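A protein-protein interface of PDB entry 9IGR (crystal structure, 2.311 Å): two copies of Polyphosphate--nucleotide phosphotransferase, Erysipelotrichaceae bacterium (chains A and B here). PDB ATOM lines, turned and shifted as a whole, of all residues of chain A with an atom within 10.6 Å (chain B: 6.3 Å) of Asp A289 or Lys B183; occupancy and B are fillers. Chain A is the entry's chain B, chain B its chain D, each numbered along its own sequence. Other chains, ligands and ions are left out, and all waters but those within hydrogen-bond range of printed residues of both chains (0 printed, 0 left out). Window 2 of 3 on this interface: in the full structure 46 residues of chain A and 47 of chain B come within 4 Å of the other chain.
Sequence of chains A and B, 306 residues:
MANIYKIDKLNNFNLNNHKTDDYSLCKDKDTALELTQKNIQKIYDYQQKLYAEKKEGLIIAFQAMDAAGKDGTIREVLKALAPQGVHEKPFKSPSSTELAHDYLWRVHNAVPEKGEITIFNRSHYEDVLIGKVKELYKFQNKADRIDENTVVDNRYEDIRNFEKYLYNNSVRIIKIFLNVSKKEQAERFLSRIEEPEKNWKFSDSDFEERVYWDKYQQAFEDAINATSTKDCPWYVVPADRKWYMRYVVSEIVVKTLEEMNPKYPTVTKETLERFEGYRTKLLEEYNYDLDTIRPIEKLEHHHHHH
The side-chain hydroxyl (OH) of Tyr A286 lies within hydrogen-bond range of the guanidinium group (NH2) of Arg B210, at 3.0 Å.
The side-chain carboxylate of Glu A285 lies within salt-bridge range of the guanidinium group of Arg B210 (3.1 Å).
N of Asp A291 lies within hydrogen-bond range of OE1 of Glu B187 (3.0 Å).
The side-chain amino group of Lys B182 is in salt-bridge range of the side-chain carboxylate of Glu A285 (3.6 Å).
The side-chain carboxylate of Asp A289 lies within salt-bridge range of the side-chain amino group of Lys B183, 2.5 Å away.
The side-chain amide oxygen (OE1) of Gln B185 sits at hydrogen-bond distance from the guanidinium group (NH1) of Arg B210 (3.0 Å).
O of Lys B182 lies within hydrogen-bond range of NH1 of Arg B210, 3.1 Å away.
The backbone carbonyl oxygen (O) of Leu A290 is in hydrogen-bond range of the side-chain amino group (NZ) of Lys A298 (2.9 Å).
Arg B210 touches Leu A282.
Lys B182 touches Tyr A286.
Lys B183 touches Tyr A286 (CD to CD1, 3.5 Å).
CE2 of Tyr A286 touches CB of Ala B186 (3.6 Å).
Asp A289 touches Glu B187 (O to OE2, 3.9 Å).
Glu B187 touches Leu A290 (OE2 to CD2, 3.5 Å).
Of chain B, only Lys B183 and Glu B187 come within 4 Å of Asp A289.
Of the printed residues of chain B, Leu A290 touches Glu B187 (3.5 Å).
Lys B183 touches just these residues of chain A: Tyr A286 and Asp A289.
Gln B185 touches none of the printed residues of chain A.
Of the printed residues of chain A, Ala B186 touches Tyr A286.
Glu B187 touches just these residues of chain A: Asp A289 (3.9 Å), Leu A290 (3.5 Å) and Asp A291 (3.0 Å).
The nearest printed residue of chain B that does not touch Asp A289 is Ala B186 (8.0 Å).
The nearest printed residue of chain B that does not touch Leu A282 is Ala B186 (4.0004 Å).
Of the 10 printed residues of chain B, 5 touch a printed residue of chain A.
Hydrophobic or aromatic side chains of chain B that line the printed part of chain A: Ala B186.
Among the printed residues, 11 pairs touch across the chains.
No position is printed for both chains.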
ATOM      1  N   ARG A 279      30.732  12.734  -2.582  1.00  0.00           N
ATOM      2  CA  ARG A 279      30.479  11.599  -1.706  1.00  0.00           C
ATOM      3  C   ARG A 279      29.068  11.030  -1.841  1.00  0.00           C
ATOM      4  O   ARG A 279      28.877   9.826  -1.935  1.00  0.00           O
ATOM      5  CB  ARG A 279      30.826  12.003  -0.266  1.00  0.00           C
ATOM      6  CG  ARG A 279      30.340  11.049   0.808  1.00  0.00           C
ATOM      7  CD  ARG A 279      30.821  11.517   2.182  1.00  0.00           C
ATOM      8  NE  ARG A 279      30.481  10.533   3.216  1.00  0.00           N
ATOM      9  CZ  ARG A 279      29.289  10.317   3.718  1.00  0.00           C
ATOM     10  NH1 ARG A 279      28.305  11.127   3.451  1.00  0.00           N
ATOM     11  NH2 ARG A 279      29.075   9.290   4.511  1.00  0.00           N
ATOM     12  N   THR A 280      28.055  11.874  -1.815  1.00  0.00           N
ATOM     13  CA  THR A 280      26.678  11.413  -1.935  1.00  0.00           C
ATOM     14  C   THR A 280      26.492  10.705  -3.278  1.00  0.00           C
ATOM     15  O   THR A 280      25.857   9.645  -3.322  1.00  0.00           O
ATOM     16  CB  THR A 280      25.727  12.601  -1.830  1.00  0.00           C
ATOM     17  OG1 THR A 280      26.098  13.242  -0.628  1.00  0.00           O
ATOM     18  CG2 THR A 280      24.262  12.223  -1.744  1.00  0.00           C
ATOM     19  N   LYS A 281      27.078  11.266  -4.353  1.00  0.00           N
ATOM     20  CA  LYS A 281      26.946  10.682  -5.678  1.00  0.00           C
ATOM     21  C   LYS A 281      27.539   9.269  -5.717  1.00  0.00           C
ATOM     22  O   LYS A 281      26.928   8.327  -6.236  1.00  0.00           O
ATOM     23  CB  LYS A 281      27.688  11.480  -6.749  1.00  0.00           C
ATOM     24  CG  LYS A 281      27.200  12.876  -6.974  1.00  0.00           C
ATOM     25  CD  LYS A 281      25.964  12.833  -7.842  1.00  0.00           C
ATOM     26  CE  LYS A 281      25.273  14.128  -7.934  1.00  0.00           C
ATOM     27  NZ  LYS A 281      23.989  13.699  -8.520  1.00  0.00           N
ATOM     28  N   LEU A 282      28.732   9.133  -5.146  1.00  0.00           N
ATOM     29  CA  LEU A 282      29.406   7.843  -5.154  1.00  0.00           C
ATOM     30  C   LEU A 282      28.629   6.841  -4.329  1.00  0.00           C
ATOM     31  O   LEU A 282      28.461   5.721  -4.772  1.00  0.00           O
ATOM     32  CB  LEU A 282      30.783   8.007  -4.600  1.00  0.00           C
ATOM     33  CG  LEU A 282      31.732   8.811  -5.490  1.00  0.00           C
ATOM     34  CD1 LEU A 282      33.042   9.138  -4.746  1.00  0.00           C
ATOM     35  CD2 LEU A 282      31.974   8.030  -6.781  1.00  0.00           C
ATOM     36  N   LEU A 283      28.099   7.290  -3.189  1.00  0.00           N
ATOM     37  CA  LEU A 283      27.313   6.429  -2.355  1.00  0.00           C
ATOM     38  C   LEU A 283      26.070   6.038  -3.116  1.00  0.00           C
ATOM     39  O   LEU A 283      25.695   4.871  -3.096  1.00  0.00           O
ATOM     40  CB  LEU A 283      27.022   7.073  -1.006  1.00  0.00           C
ATOM     41  CG  LEU A 283      28.213   7.168  -0.030  1.00  0.00           C
ATOM     42  CD1 LEU A 283      27.985   8.171   1.077  1.00  0.00           C
ATOM     43  CD2 LEU A 283      28.542   5.819   0.586  1.00  0.00           C
ATOM     44  N   GLU A 284      25.424   6.982  -3.799  1.00  0.00           N
ATOM     45  CA  GLU A 284      24.182   6.652  -4.507  1.00  0.00           C
ATOM     46  C   GLU A 284      24.469   5.684  -5.650  1.00  0.00           C
ATOM     47  O   GLU A 284      23.761   4.718  -5.813  1.00  0.00           O
ATOM     48  CB  GLU A 284      23.447   7.874  -5.031  1.00  0.00           C
ATOM     49  CG  GLU A 284      22.729   8.646  -3.932  1.00  0.00           C
ATOM     50  CD  GLU A 284      22.300  10.093  -4.262  1.00  0.00           C
ATOM     51  OE1 GLU A 284      22.661  10.628  -5.341  1.00  0.00           O
ATOM     52  OE2 GLU A 284      21.592  10.738  -3.417  1.00  0.00           O
ATOM     53  N   GLU A 285      25.580   5.859  -6.361  1.00  0.00           N
ATOM     54  CA  GLU A 285      25.905   4.960  -7.449  1.00  0.00           C
ATOM     55  C   GLU A 285      25.928   3.534  -6.948  1.00  0.00           C
ATOM     56  O   GLU A 285      25.567   2.637  -7.662  1.00  0.00           O
ATOM     57  CB  GLU A 285      27.204   5.415  -8.098  1.00  0.00           C
ATOM     58  CG  GLU A 285      27.454   4.904  -9.512  1.00  0.00           C
ATOM     59  CD  GLU A 285      28.831   5.228 -10.118  1.00  0.00           C
ATOM     60  OE1 GLU A 285      29.446   6.215  -9.645  1.00  0.00           O
ATOM     61  OE2 GLU A 285      29.331   4.491 -11.033  1.00  0.00           O
ATOM     62  N   TYR A 286      26.340   3.311  -5.704  1.00  0.00           N
ATOM     63  CA  TYR A 286      26.508   1.970  -5.181  1.00  0.00           C
ATOM     64  C   TYR A 286      25.471   1.611  -4.103  1.00  0.00           C
ATOM     65  O   TYR A 286      25.651   0.560  -3.478  1.00  0.00           O
ATOM     66  CB  TYR A 286      27.969   1.785  -4.733  1.00  0.00           C
ATOM     67  CG  TYR A 286      28.931   1.894  -5.897  1.00  0.00           C
ATOM     68  CD1 TYR A 286      29.108   0.859  -6.813  1.00  0.00           C
ATOM     69  CD2 TYR A 286      29.653   3.042  -6.107  1.00  0.00           C
ATOM     70  CE1 TYR A 286      29.869   1.008  -7.965  1.00  0.00           C
ATOM     71  CE2 TYR A 286      30.474   3.189  -7.218  1.00  0.00           C
ATOM     72  CZ  TYR A 286      30.602   2.159  -8.122  1.00  0.00           C
ATOM     73  OH  TYR A 286      31.383   2.286  -9.224  1.00  0.00           O
ATOM     74  N   ASN A 287      24.348   2.381  -3.994  1.00  0.00           N
ATOM     75  CA  ASN A 287      23.322   2.266  -2.944  1.00  0.00           C
ATOM     76  C   ASN A 287      23.965   2.041  -1.570  1.00  0.00           C
ATOM     77  O   ASN A 287      23.727   1.065  -0.878  1.00  0.00           O
ATOM     78  CB  ASN A 287      22.141   1.328  -3.265  1.00  0.00           C
ATOM     79  CG  ASN A 287      21.229   1.824  -4.424  1.00  0.00           C
ATOM     80  OD1 ASN A 287      20.435   1.048  -4.954  1.00  0.00           O
ATOM     81  ND2 ASN A 287      21.257   3.080  -4.908  1.00  0.00           N
ATOM     82  N   TYR A 288      24.838   2.967  -1.223  1.00  0.00           N
ATOM     83  CA  TYR A 288      25.465   3.059   0.081  1.00  0.00           C
ATOM     84  C   TYR A 288      26.261   1.807   0.427  1.00  0.00           C
ATOM     85  O   TYR A 288      26.724   1.700   1.532  1.00  0.00           O
ATOM     86  CB  TYR A 288      24.357   3.475   1.050  1.00  0.00           C
ATOM     87  CG  TYR A 288      24.067   4.960   0.916  1.00  0.00           C
ATOM     88  CD1 TYR A 288      23.221   5.435  -0.078  1.00  0.00           C
ATOM     89  CD2 TYR A 288      24.664   5.876   1.766  1.00  0.00           C
ATOM     90  CE1 TYR A 288      22.984   6.791  -0.228  1.00  0.00           C
ATOM     91  CE2 TYR A 288      24.367   7.227   1.684  1.00  0.00           C
ATOM     92  CZ  TYR A 288      23.535   7.681   0.667  1.00  0.00           C
ATOM     93  OH  TYR A 288      23.273   8.979   0.466  1.00  0.00           O
ATOM     94  N   ASP A 289      26.640   0.983  -0.545  1.00  0.00           N
ATOM     95  CA  ASP A 289      27.489  -0.162  -0.258  1.00  0.00           C
ATOM     96  C   ASP A 289      28.971   0.135  -0.485  1.00  0.00           C
ATOM     97  O   ASP A 289      29.684  -0.561  -1.205  1.00  0.00           O
ATOM     98  CB  ASP A 289      27.081  -1.350  -1.076  1.00  0.00           C
ATOM     99  CG  ASP A 289      27.868  -2.584  -0.715  1.00  0.00           C
ATOM    100  OD1 ASP A 289      27.992  -2.884   0.509  1.00  0.00           O
ATOM    101  OD2 ASP A 289      28.443  -3.144  -1.659  1.00  0.00           O
ATOM    102  N   LEU A 290      29.451   1.172   0.183  1.00  0.00           N
ATOM    103  CA  LEU A 290      30.845   1.524   0.268  1.00  0.00           C
ATOM    104  C   LEU A 290      31.183   1.624   1.749  1.00  0.00           C
ATOM    105  O   LEU A 290      30.309   1.808   2.589  1.00  0.00           O
ATOM    106  CB  LEU A 290      31.080   2.882  -0.412  1.00  0.00           C
ATOM    107  CG  LEU A 290      30.788   3.030  -1.911  1.00  0.00           C
ATOM    108  CD1 LEU A 290      30.991   4.433  -2.503  1.00  0.00           C
ATOM    109  CD2 LEU A 290      31.695   2.118  -2.705  1.00  0.00           C
ATOM    110  N   ASP A 291      32.480   1.671   2.072  1.00  0.00           N
ATOM    111  CA  ASP A 291      32.969   1.662   3.443  1.00  0.00           C
ATOM    112  C   ASP A 291      32.975   3.073   4.064  1.00  0.00           C
ATOM    113  O   ASP A 291      34.005   3.612   4.420  1.00  0.00           O
ATOM    114  CB  ASP A 291      34.353   1.016   3.383  1.00  0.00           C
ATOM    115  CG  ASP A 291      35.305   1.019   4.590  1.00  0.00           C
ATOM    116  OD1 ASP A 291      34.907   0.382   5.587  1.00  0.00           O
ATOM    117  OD2 ASP A 291      36.481   1.602   4.507  1.00  0.00           O
ATOM    118  N   THR A 292      31.854   3.682   4.343  1.00  0.00           N
ATOM    119  CA  THR A 292      31.963   5.052   4.778  1.00  0.00           C
ATOM    120  C   THR A 292      32.402   5.013   6.243  1.00  0.00           C
ATOM    121  O   THR A 292      32.069   4.125   6.983  1.00  0.00           O
ATOM    122  CB  THR A 292      30.640   5.795   4.545  1.00  0.00           C
ATOM    123  OG1 THR A 292      30.727   7.038   5.259  1.00  0.00           O
ATOM    124  CG2 THR A 292      29.434   5.008   5.034  1.00  0.00           C
ATOM    125  N   ILE A 293      33.063   6.063   6.690  1.00  0.00           N
ATOM    126  CA  ILE A 293      33.348   6.283   8.086  1.00  0.00           C
ATOM    127  C   ILE A 293      32.129   6.797   8.851  1.00  0.00           C
ATOM    128  O   ILE A 293      32.303   7.163  10.002  1.00  0.00           O
ATOM    129  CB  ILE A 293      34.558   7.229   8.142  1.00  0.00           C
ATOM    130  CG1 ILE A 293      35.605   6.574   8.910  1.00  0.00           C
ATOM    131  CG2 ILE A 293      34.288   8.662   8.594  1.00  0.00           C
ATOM    132  CD1 ILE A 293      35.940   5.196   8.355  1.00  0.00           C
ATOM    133  N   ARG A 294      30.941   6.823   8.235  1.00  0.00           N
ATOM    134  CA  ARG A 294      29.738   7.343   8.877  1.00  0.00           C
ATOM    135  C   ARG A 294      28.609   6.340   8.719  1.00  0.00           C
ATOM    136  O   ARG A 294      27.615   6.631   8.093  1.00  0.00           O
ATOM    137  CB  ARG A 294      29.200   8.680   8.348  1.00  0.00           C
ATOM    138  CG  ARG A 294      30.188   9.829   8.538  1.00  0.00           C
ATOM    139  CD  ARG A 294      29.714  11.193   8.037  1.00  0.00           C
ATOM    140  NE  ARG A 294      30.946  11.745   7.449  1.00  0.00           N
ATOM    141  CZ  ARG A 294      31.020  12.691   6.505  1.00  0.00           C
ATOM    142  NH1 ARG A 294      29.938  13.279   6.065  1.00  0.00           N
ATOM    143  NH2 ARG A 294      32.163  13.021   5.942  1.00  0.00           N
ATOM    144  N   PRO A 295      28.683   5.140   9.315  1.00  0.00           N
ATOM    145  CA  PRO A 295      27.738   4.079   8.956  1.00  0.00           C
ATOM    146  C   PRO A 295      26.268   4.338   9.306  1.00  0.00           C
ATOM    147  O   PRO A 295      25.454   3.626   8.737  1.00  0.00           O
ATOM    148  CB  PRO A 295      28.397   2.807   9.554  1.00  0.00           C
ATOM    149  CG  PRO A 295      29.824   3.247   9.944  1.00  0.00           C
ATOM    150  CD  PRO A 295      29.709   4.708  10.282  1.00  0.00           C
ATOM    151  N   GLU A 297      24.242   6.789   8.323  1.00  0.00           N
ATOM    152  CA  GLU A 297      23.637   7.155   7.052  1.00  0.00           C
ATOM    153  C   GLU A 297      23.184   5.955   6.194  1.00  0.00           C
ATOM    154  O   GLU A 297      22.112   6.010   5.595  1.00  0.00           O
ATOM    155  CB  GLU A 297      24.705   7.890   6.246  1.00  0.00           C
ATOM    156  CG  GLU A 297      24.996   9.345   6.618  1.00  0.00           C
ATOM    157  CD  GLU A 297      25.473  10.084   5.375  1.00  0.00           C
ATOM    158  OE1 GLU A 297      24.725  10.054   4.351  1.00  0.00           O
ATOM    159  OE2 GLU A 297      26.572  10.663   5.409  1.00  0.00           O
ATOM    160  N   LYS A 298      23.964   4.863   6.157  1.00  0.00           N
ATOM    161  CA  LYS A 298      23.564   3.619   5.498  1.00  0.00           C
ATOM    162  C   LYS A 298      22.220   3.048   5.916  1.00  0.00           C
ATOM    163  O   LYS A 298      21.634   2.428   5.034  1.00  0.00           O
ATOM    164  CB  LYS A 298      24.545   2.457   5.656  1.00  0.00           C
ATOM    165  CG  LYS A 298      25.883   2.875   5.165  1.00  0.00           C
ATOM    166  CD  LYS A 298      26.990   1.855   5.324  1.00  0.00           C
ATOM    167  CE  LYS A 298      26.977   0.653   4.414  1.00  0.00           C
ATOM    168  NZ  LYS A 298      28.415   0.366   4.284  1.00  0.00           N
ATOM    169  N   LEU A 299      21.725   3.287   7.159  1.00  0.00           N
ATOM    170  CA  LEU A 299      20.485   2.700   7.684  1.00  0.00           C
ATOM    171  C   LEU A 299      19.221   3.175   6.966  1.00  0.00           C
ATOM    172  O   LEU A 299      18.225   2.427   6.927  1.00  0.00           O
ATOM    173  CB  LEU A 299      20.319   2.964   9.186  1.00  0.00           C
ATOM    174  CG  LEU A 299      20.975   2.001  10.185  1.00  0.00           C
ATOM    175  CD1 LEU A 299      22.222   1.363   9.638  1.00  0.00           C
ATOM    176  CD2 LEU A 299      21.308   2.763  11.479  1.00  0.00           C
ATOM    177  N   HIS A 301      18.744   3.556   3.692  1.00  0.00           N
ATOM    178  CA  HIS A 301      18.798   3.357   2.242  1.00  0.00           C
ATOM    179  C   HIS A 301      18.544   1.888   1.895  1.00  0.00           C
ATOM    180  O   HIS A 301      18.916   1.127   2.768  1.00  0.00           O
ATOM    181  CB  HIS A 301      20.132   4.001   1.793  1.00  0.00           C
ATOM    182  CG  HIS A 301      20.118   5.521   1.845  1.00  0.00           C
ATOM    183  ND1 HIS A 301      21.024   6.241   2.583  1.00  0.00           N
ATOM    184  CD2 HIS A 301      19.269   6.460   1.331  1.00  0.00           C
ATOM    185  CE1 HIS A 301      20.775   7.555   2.501  1.00  0.00           C
ATOM    186  NE2 HIS A 301      19.709   7.702   1.744  1.00  0.00           N
ATOM    187  N   HIS A 302      17.845   1.533   0.744  1.00  0.00           N
ATOM    188  CA  HIS A 302      17.750   0.193   0.087  1.00  0.00           C
ATOM    189  C   HIS A 302      16.432   0.048  -0.770  1.00  0.00           C
ATOM    190  O   HIS A 302      15.786  -1.084  -1.283  1.00  0.00           O
ATOM    191  CB  HIS A 302      18.081  -0.985   1.055  1.00  0.00           C
ATOM    192  CG  HIS A 302      18.182  -2.455   0.595  1.00  0.00           C
ATOM    193  ND1 HIS A 302      19.349  -3.211   0.640  1.00  0.00           N
ATOM    194  CD2 HIS A 302      17.208  -3.355   0.212  1.00  0.00           C
ATOM    195  CE1 HIS A 302      19.105  -4.453   0.186  1.00  0.00           C
ATOM    196  NE2 HIS A 302      17.814  -4.557  -0.101  1.00  0.00           N
ATOM    197  N   SER B 181      39.057  -1.936 -10.366  1.00  0.00           N
ATOM    198  CA  SER B 181      37.655  -1.892 -10.771  1.00  0.00           C
ATOM    199  C   SER B 181      37.119  -0.508 -10.420  1.00  0.00           C
ATOM    200  O   SER B 181      37.663   0.154  -9.533  1.00  0.00           O
ATOM    201  CB  SER B 181      36.837  -2.893  -9.983  1.00  0.00           C
ATOM    202  OG  SER B 181      36.914  -2.657  -8.563  1.00  0.00           O
ATOM    203  N   LYS B 182      36.019  -0.118 -11.044  1.00  0.00           N
ATOM    204  CA  LYS B 182      35.431   1.172 -10.797  1.00  0.00           C
ATOM    205  C   LYS B 182      34.845   1.269  -9.373  1.00  0.00           C
ATOM    206  O   LYS B 182      34.965   2.333  -8.734  1.00  0.00           O
ATOM    207  CB  LYS B 182      34.368   1.327 -11.881  1.00  0.00           C
ATOM    208  CG  LYS B 182      33.790   2.680 -12.045  1.00  0.00           C
ATOM    209  CD  LYS B 182      32.720   2.669 -13.134  1.00  0.00           C
ATOM    210  CE  LYS B 182      32.286   4.106 -13.378  1.00  0.00           C
ATOM    211  NZ  LYS B 182      31.064   4.044 -14.158  1.00  0.00           N
ATOM    212  N   LYS B 183      34.260   0.194  -8.842  1.00  0.00           N
ATOM    213  CA  LYS B 183      33.790   0.263  -7.471  1.00  0.00           C
ATOM    214  C   LYS B 183      34.959   0.438  -6.495  1.00  0.00           C
ATOM    215  O   LYS B 183      34.898   1.221  -5.540  1.00  0.00           O
ATOM    216  CB  LYS B 183      32.792  -0.806  -7.034  1.00  0.00           C
ATOM    217  CG  LYS B 183      32.559  -0.924  -5.506  1.00  0.00           C
ATOM    218  CD  LYS B 183      31.189  -1.450  -5.136  1.00  0.00           C
ATOM    219  CE  LYS B 183      31.096  -1.984  -3.765  1.00  0.00           C
ATOM    220  NZ  LYS B 183      29.750  -2.598  -3.759  1.00  0.00           N
ATOM    221  N   GLU B 184      36.061  -0.250  -6.715  1.00  0.00           N
ATOM    222  CA  GLU B 184      37.138  -0.058  -5.762  1.00  0.00           C
ATOM    223  C   GLU B 184      37.711   1.362  -5.856  1.00  0.00           C
ATOM    224  O   GLU B 184      38.120   1.925  -4.869  1.00  0.00           O
ATOM    225  CB  GLU B 184      38.232  -1.115  -5.983  1.00  0.00           C
ATOM    226  CG  GLU B 184      39.349  -1.044  -4.938  1.00  0.00           C
ATOM    227  CD  GLU B 184      39.038  -1.222  -3.430  1.00  0.00           C
ATOM    228  OE1 GLU B 184      37.974  -1.811  -3.185  1.00  0.00           O
ATOM    229  OE2 GLU B 184      39.879  -0.830  -2.513  1.00  0.00           O
ATOM    230  N   GLN B 185      37.764   1.953  -7.056  1.00  0.00           N
ATOM    231  CA  GLN B 185      38.183   3.319  -7.222  1.00  0.00           C
ATOM    232  C   GLN B 185      37.279   4.220  -6.401  1.00  0.00           C
ATOM    233  O   GLN B 185      37.710   5.102  -5.671  1.00  0.00           O
ATOM    234  CB  GLN B 185      38.218   3.769  -8.693  1.00  0.00           C
ATOM    235  CG  GLN B 185      38.599   5.231  -8.869  1.00  0.00           C
ATOM    236  CD  GLN B 185      38.383   5.744 -10.275  1.00  0.00           C
ATOM    237  OE1 GLN B 185      37.283   5.968 -10.786  1.00  0.00           O
ATOM    238  NE2 GLN B 185      39.489   6.030 -10.906  1.00  0.00           N
ATOM    239  N   ALA B 186      36.000   3.946  -6.437  1.00  0.00           N
ATOM    240  CA  ALA B 186      35.092   4.788  -5.693  1.00  0.00           C
ATOM    241  C   ALA B 186      35.347   4.652  -4.210  1.00  0.00           C
ATOM    242  O   ALA B 186      35.238   5.640  -3.502  1.00  0.00           O
ATOM    243  CB  ALA B 186      33.667   4.479  -6.055  1.00  0.00           C
ATOM    244  N   GLU B 187      35.704   3.470  -3.722  1.00  0.00           N
ATOM    245  CA  GLU B 187      35.908   3.360  -2.293  1.00  0.00           C
ATOM    246  C   GLU B 187      37.130   4.191  -1.914  1.00  0.00           C
ATOM    247  O   GLU B 187      37.189   4.856  -0.893  1.00  0.00           O
ATOM    248  CB  GLU B 187      36.303   1.943  -1.846  1.00  0.00           C
ATOM    249  CG  GLU B 187      35.295   0.831  -2.094  1.00  0.00           C
ATOM    250  CD  GLU B 187      34.427   0.593  -0.900  1.00  0.00           C
ATOM    251  OE1 GLU B 187      34.740   1.318   0.101  1.00  0.00           O
ATOM    252  OE2 GLU B 187      33.558  -0.355  -1.009  1.00  0.00           O
ATOM    253  N   ARG B 188      38.159   4.140  -2.739  1.00  0.00           N
ATOM    254  CA  ARG B 188      39.367   4.862  -2.416  1.00  0.00           C
ATOM    255  C   ARG B 188      39.123   6.363  -2.558  1.00  0.00           C
ATOM    256  O   ARG B 188      39.744   7.120  -1.813  1.00  0.00           O
ATOM    257  CB  ARG B 188      40.463   4.381  -3.355  1.00  0.00           C
ATOM    258  CG  ARG B 188      40.883   2.973  -2.975  1.00  0.00           C
ATOM    259  CD  ARG B 188      41.890   2.396  -3.965  1.00  0.00           C
ATOM    260  NE  ARG B 188      42.113   0.947  -3.770  1.00  0.00           N
ATOM    261  CZ  ARG B 188      42.840   0.168  -4.503  1.00  0.00           C
ATOM    262  NH1 ARG B 188      43.391   0.630  -5.598  1.00  0.00           N
ATOM    263  NH2 ARG B 188      42.925  -1.113  -4.220  1.00  0.00           N
ATOM    264  N   ARG B 210      35.334   9.670 -14.362  1.00  0.00           N
ATOM    265  CA  ARG B 210      34.638   8.398 -14.219  1.00  0.00           C
ATOM    266  C   ARG B 210      33.697   8.136 -15.393  1.00  0.00           C
ATOM    267  O   ARG B 210      33.584   7.027 -15.879  1.00  0.00           O
ATOM    268  CB  ARG B 210      33.909   8.288 -12.893  1.00  0.00           C
ATOM    269  CG  ARG B 210      34.897   7.898 -11.805  1.00  0.00           C
ATOM    270  CD  ARG B 210      34.329   8.046 -10.428  1.00  0.00           C
ATOM    271  NE  ARG B 210      33.276   7.066 -10.143  1.00  0.00           N
ATOM    272  CZ  ARG B 210      33.401   5.777  -9.870  1.00  0.00           C
ATOM    273  NH1 ARG B 210      34.593   5.221  -9.719  1.00  0.00           N
ATOM    274  NH2 ARG B 210      32.322   5.066  -9.682  1.00  0.00           N
ATOM    275  N   TRP B 213      34.985   5.950 -18.127  1.00  0.00           N
ATOM    276  CA  TRP B 213      35.621   4.725 -17.656  1.00  0.00           C
ATOM    277  C   TRP B 213      35.813   3.701 -18.768  1.00  0.00           C
ATOM    278  O   TRP B 213      36.915   3.164 -18.950  1.00  0.00           O
ATOM    279  CB  TRP B 213      34.794   4.129 -16.510  1.00  0.00           C
ATOM    280  CG  TRP B 213      35.426   2.885 -15.979  1.00  0.00           C
ATOM    281  CD1 TRP B 213      35.138   1.596 -16.349  1.00  0.00           C
ATOM    282  CD2 TRP B 213      36.450   2.831 -14.968  1.00  0.00           C
ATOM    283  NE1 TRP B 213      35.939   0.755 -15.643  1.00  0.00           N
ATOM    284  CE2 TRP B 213      36.748   1.470 -14.795  1.00  0.00           C
ATOM    285  CE3 TRP B 213      37.111   3.776 -14.202  1.00  0.00           C
ATOM    286  CZ2 TRP B 213      37.703   1.040 -13.884  1.00  0.00           C
ATOM    287  CZ3 TRP B 213      38.034   3.362 -13.291  1.00  0.00           C
ATOM    288  CH2 TRP B 213      38.362   1.997 -13.149  1.00  0.00           C
